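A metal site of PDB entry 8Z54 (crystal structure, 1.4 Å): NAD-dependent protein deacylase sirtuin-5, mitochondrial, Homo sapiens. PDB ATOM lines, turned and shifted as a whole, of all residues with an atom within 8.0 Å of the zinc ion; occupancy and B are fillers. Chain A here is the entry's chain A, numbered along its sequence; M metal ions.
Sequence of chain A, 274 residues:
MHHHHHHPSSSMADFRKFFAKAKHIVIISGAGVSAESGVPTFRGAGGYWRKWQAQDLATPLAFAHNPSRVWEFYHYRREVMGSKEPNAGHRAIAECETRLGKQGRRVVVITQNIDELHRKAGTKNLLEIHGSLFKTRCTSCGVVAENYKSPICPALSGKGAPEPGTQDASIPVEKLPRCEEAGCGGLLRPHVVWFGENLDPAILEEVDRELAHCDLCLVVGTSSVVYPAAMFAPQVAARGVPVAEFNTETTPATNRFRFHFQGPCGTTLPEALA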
ATOM      1  N   ARG A 137      22.858 -13.265  15.167  1.00  0.00           N
ATOM      2  CA  ARG A 137      21.692 -13.720  15.910  1.00  0.00           C
ATOM      3  C   ARG A 137      20.438 -13.126  15.270  1.00  0.00           C
ATOM      4  O   ARG A 137      20.391 -11.915  15.013  1.00  0.00           O
ATOM      5  CB  ARG A 137      21.802 -13.256  17.385  1.00  0.00           C
ATOM      6  CG  ARG A 137      20.765 -13.864  18.287  1.00  0.00           C
ATOM      7  CD  ARG A 137      20.769 -13.152  19.740  1.00  0.00           C
ATOM      8  NE  ARG A 137      22.105 -12.803  20.234  1.00  0.00           N
ATOM      9  CZ  ARG A 137      22.329 -11.854  21.121  1.00  0.00           C
ATOM     10  NH1 ARG A 137      21.341 -11.047  21.525  1.00  0.00           N
ATOM     11  NH2 ARG A 137      23.565 -11.692  21.609  1.00  0.00           N
ATOM     12  N   CYS A 138      19.436 -13.959  15.032  1.00  0.00           N
ATOM     13  CA  CYS A 138      18.186 -13.499  14.446  1.00  0.00           C
ATOM     14  C   CYS A 138      17.309 -12.814  15.515  1.00  0.00           C
ATOM     15  O   CYS A 138      17.048 -13.385  16.572  1.00  0.00           O
ATOM     16  CB  CYS A 138      17.434 -14.656  13.773  1.00  0.00           C
ATOM     17  SG  CYS A 138      15.910 -14.047  13.028  1.00  0.00           S
ATOM     18  N   THR A 139      16.885 -11.583  15.220  1.00  0.00           N
ATOM     19  CA  THR A 139      16.036 -10.829  16.149  1.00  0.00           C
ATOM     20  C   THR A 139      14.584 -11.288  16.141  1.00  0.00           C
ATOM     21  O   THR A 139      13.811 -10.787  16.969  1.00  0.00           O
ATOM     22  CB  THR A 139      16.120  -9.300  15.875  1.00  0.00           C
ATOM     23  OG1 THR A 139      15.595  -9.015  14.568  1.00  0.00           O
ATOM     24  CG2 THR A 139      17.571  -8.806  16.009  1.00  0.00           C
ATOM     25  N   SER A 140      14.208 -12.209  15.252  1.00  0.00           N
ATOM     26  CA  SER A 140      12.876 -12.836  15.239  1.00  0.00           C
ATOM     27  C   SER A 140      12.907 -14.204  15.918  1.00  0.00           C
ATOM     28  O   SER A 140      12.259 -14.418  16.942  1.00  0.00           O
ATOM     29  CB  SER A 140      12.301 -12.977  13.811  1.00  0.00           C
ATOM     30  OG  SER A 140      11.911 -11.719  13.304  1.00  0.00           O
ATOM     31  N   CYS A 141      13.684 -15.142  15.369  1.00  0.00           N
ATOM     32  CA  CYS A 141      13.664 -16.514  15.852  1.00  0.00           C
ATOM     33  C   CYS A 141      14.772 -16.843  16.856  1.00  0.00           C
ATOM     34  O   CYS A 141      14.741 -17.924  17.455  1.00  0.00           O
ATOM     35  CB  CYS A 141      13.702 -17.496  14.676  1.00  0.00           C
ATOM     36  SG  CYS A 141      15.322 -17.656  13.866  1.00  0.00           S
ATOM     37  N   GLY A 142      15.757 -15.951  17.034  1.00  0.00           N
ATOM     38  CA  GLY A 142      16.828 -16.165  18.002  1.00  0.00           C
ATOM     39  C   GLY A 142      17.930 -17.132  17.592  1.00  0.00           C
ATOM     40  O   GLY A 142      18.840 -17.367  18.408  1.00  0.00           O
ATOM     41  N   VAL A 143      17.895 -17.696  16.378  1.00  0.00           N
ATOM     42  CA  VAL A 143      18.919 -18.658  15.960  1.00  0.00           C
ATOM     43  C   VAL A 143      20.259 -17.952  15.831  1.00  0.00           C
ATOM     44  O   VAL A 143      20.359 -16.845  15.283  1.00  0.00           O
ATOM     45  CB  VAL A 143      18.539 -19.371  14.656  1.00  0.00           C
ATOM     46  CG1 VAL A 143      18.543 -18.410  13.487  1.00  0.00           C
ATOM     47  CG2 VAL A 143      19.559 -20.432  14.345  1.00  0.00           C
ATOM     48  N   VAL A 144      21.306 -18.614  16.315  1.00  0.00           N
ATOM     49  CA  VAL A 144      22.672 -18.116  16.232  1.00  0.00           C
ATOM     50  C   VAL A 144      23.374 -18.887  15.127  1.00  0.00           C
ATOM     51  O   VAL A 144      23.177 -20.106  15.001  1.00  0.00           O
ATOM     52  CB  VAL A 144      23.375 -18.330  17.600  1.00  0.00           C
ATOM     53  CG1 VAL A 144      24.837 -18.013  17.486  1.00  0.00           C
ATOM     54  CG2 VAL A 144      22.695 -17.515  18.668  1.00  0.00           C
ATOM     55  N   ARG A 178      19.792 -10.857   6.637  1.00  0.00           N
ATOM     56  CA  ARG A 178      18.525 -11.476   6.976  1.00  0.00           C
ATOM     57  C   ARG A 178      18.692 -12.971   7.267  1.00  0.00           C
ATOM     58  O   ARG A 178      19.556 -13.639   6.688  1.00  0.00           O
ATOM     59  CB  ARG A 178      17.501 -11.285   5.854  1.00  0.00           C
ATOM     60  CG  ARG A 178      17.428  -9.867   5.277  1.00  0.00           C
ATOM     61  CD  ARG A 178      16.924  -8.843   6.277  1.00  0.00           C
ATOM     62  NE  ARG A 178      15.643  -9.223   6.865  1.00  0.00           N
ATOM     63  CZ  ARG A 178      14.853  -8.390   7.522  1.00  0.00           C
ATOM     64  NH1 ARG A 178      15.177  -7.110   7.674  1.00  0.00           N
ATOM     65  NH2 ARG A 178      13.737  -8.851   8.075  1.00  0.00           N
ATOM     66  N   CYS A 179      17.794 -13.491   8.121  1.00  0.00           N
ATOM     67  CA  CYS A 179      17.844 -14.879   8.595  1.00  0.00           C
ATOM     68  C   CYS A 179      17.500 -15.822   7.459  1.00  0.00           C
ATOM     69  O   CYS A 179      16.497 -15.622   6.755  1.00  0.00           O
ATOM     70  CB  CYS A 179      16.833 -15.069   9.737  1.00  0.00           C
ATOM     71  SG  CYS A 179      16.880 -16.696  10.532  1.00  0.00           S
ATOM     72  N   GLU A 180      18.316 -16.855   7.277  1.00  0.00           N
ATOM     73  CA  GLU A 180      18.080 -17.794   6.186  1.00  0.00           C
ATOM     74  C   GLU A 180      17.384 -19.057   6.640  1.00  0.00           C
ATOM     75  O   GLU A 180      17.194 -19.980   5.847  1.00  0.00           O
ATOM     76  CB  GLU A 180      19.373 -18.054   5.417  1.00  0.00           C
ATOM     77  CG  GLU A 180      19.791 -16.828   4.612  1.00  0.00           C
ATOM     78  CD  GLU A 180      21.107 -16.960   3.874  1.00  0.00           C
ATOM     79  OE1 GLU A 180      21.481 -18.088   3.506  1.00  0.00           O
ATOM     80  OE2 GLU A 180      21.750 -15.902   3.637  1.00  0.00           O
ATOM     81  N   GLU A 181      16.966 -19.112   7.905  1.00  0.00           N
ATOM     82  CA  GLU A 181      16.122 -20.198   8.372  1.00  0.00           C
ATOM     83  C   GLU A 181      14.834 -20.221   7.569  1.00  0.00           C
ATOM     84  O   GLU A 181      14.133 -19.197   7.431  1.00  0.00           O
ATOM     85  CB  GLU A 181      15.836 -20.003   9.864  1.00  0.00           C
ATOM     86  CG  GLU A 181      15.909 -21.260  10.736  1.00  0.00           C
ATOM     87  CD  GLU A 181      17.252 -22.005  10.713  1.00  0.00           C
ATOM     88  OE1 GLU A 181      18.328 -21.403  10.486  1.00  0.00           O
ATOM     89  OE2 GLU A 181      17.226 -23.225  10.947  1.00  0.00           O
ATOM     90  N   ALA A 182      14.525 -21.391   7.011  1.00  0.00           N
ATOM     91  CA  ALA A 182      13.313 -21.582   6.226  1.00  0.00           C
ATOM     92  C   ALA A 182      12.130 -20.966   6.945  1.00  0.00           C
ATOM     93  O   ALA A 182      11.794 -21.358   8.063  1.00  0.00           O
ATOM     94  CB  ALA A 182      13.085 -23.083   6.035  1.00  0.00           C
ATOM     95  N   GLY A 183      11.546 -19.940   6.336  1.00  0.00           N
ATOM     96  CA  GLY A 183      10.332 -19.344   6.843  1.00  0.00           C
ATOM     97  C   GLY A 183      10.523 -18.215   7.821  1.00  0.00           C
ATOM     98  O   GLY A 183       9.536 -17.751   8.399  1.00  0.00           O
ATOM     99  N   CYS A 184      11.760 -17.747   8.050  1.00  0.00           N
ATOM    100  CA  CYS A 184      11.959 -16.621   8.955  1.00  0.00           C
ATOM    101  C   CYS A 184      12.280 -15.334   8.208  1.00  0.00           C
ATOM    102  O   CYS A 184      11.403 -14.486   8.033  1.00  0.00           O
ATOM    103  CB  CYS A 184      13.027 -16.927  10.006  1.00  0.00           C
ATOM    104  SG  CYS A 184      13.210 -15.607  11.228  1.00  0.00           S
ATOM    105  N   GLY A 185      13.516 -15.195   7.734  1.00  0.00           N
ATOM    106  CA  GLY A 185      13.922 -13.953   7.103  1.00  0.00           C
ATOM    107  C   GLY A 185      13.917 -12.725   7.997  1.00  0.00           C
ATOM    108  O   GLY A 185      13.869 -11.597   7.493  1.00  0.00           O
ATOM    109  N   GLY A 186      13.970 -12.912   9.330  1.00  0.00           N
ATOM    110  CA  GLY A 186      14.061 -11.783  10.251  1.00  0.00           C
ATOM    111  C   GLY A 186      15.380 -11.039  10.132  1.00  0.00           C
ATOM    112  O   GLY A 186      16.321 -11.480   9.485  1.00  0.00           O
ATOM    113  N   LEU A 187      15.434  -9.881  10.761  1.00  0.00           N
ATOM    114  CA  LEU A 187      16.641  -9.077  10.734  1.00  0.00           C
ATOM    115  C   LEU A 187      17.702  -9.695  11.645  1.00  0.00           C
ATOM    116  O   LEU A 187      17.450  -9.945  12.827  1.00  0.00           O
ATOM    117  CB  LEU A 187      16.312  -7.662  11.237  1.00  0.00           C
ATOM    118  CG  LEU A 187      17.465  -6.679  11.396  1.00  0.00           C
ATOM    119  CD1 LEU A 187      18.204  -6.449  10.067  1.00  0.00           C
ATOM    120  CD2 LEU A 187      16.912  -5.349  11.951  1.00  0.00           C
ATOM    121  N   LEU A 188      18.900  -9.917  11.112  1.00  0.00           N
ATOM    122  CA  LEU A 188      19.993 -10.364  11.965  1.00  0.00           C
ATOM    123  C   LEU A 188      20.662  -9.188  12.648  1.00  0.00           C
ATOM    124  O   LEU A 188      20.708  -8.062  12.128  1.00  0.00           O
ATOM    125  CB  LEU A 188      21.032 -11.100  11.104  1.00  0.00           C
ATOM    126  CG  LEU A 188      20.535 -12.319  10.320  1.00  0.00           C
ATOM    127  CD1 LEU A 188      21.623 -13.021   9.498  1.00  0.00           C
ATOM    128  CD2 LEU A 188      19.856 -13.323  11.279  1.00  0.00           C
HETATM  129 ZN    ZN M   1      15.306 -16.152  12.119  1.00  0.00          ZN
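SG of Cys 179 binds the zinc ion (2.3 Å).
The side-chain sulfur (SG) of Cys 141 binds the zinc ion (2.3 Å).
SG of Cys 184 is bound to the zinc ion, at 2.3 Å.
The zinc ion is bound by SG of Cys 138, 2.4 Å away.
The nearest printed residue that does not touch the zinc ion is Val 143 (4.2 Å).
The backbone carbonyl oxygen of Gly 186 sits at hydrogen-bond distance from the backbone NH of Cys 179.
SG of Cys 179 lies close to N of Glu 181 (3.6 Å).
The backbone carbonyl oxygen (O) of Cys 179 sits close to the backbone NH (N) of Gly 185 (3.2 Å).
N of Val 143 lies close to SG of Cys 141, 3.6 Å away.
SG of Cys 184 lies close to N of Gly 186.
The backbone NH of Cys 138 is in hydrogen-bond range of the backbone carbonyl oxygen of Val 143 (3.0 Å).
The side-chain sulfur (SG) of Cys 138 sits close to the backbone NH (N) of Ser 140 (3.3 Å).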
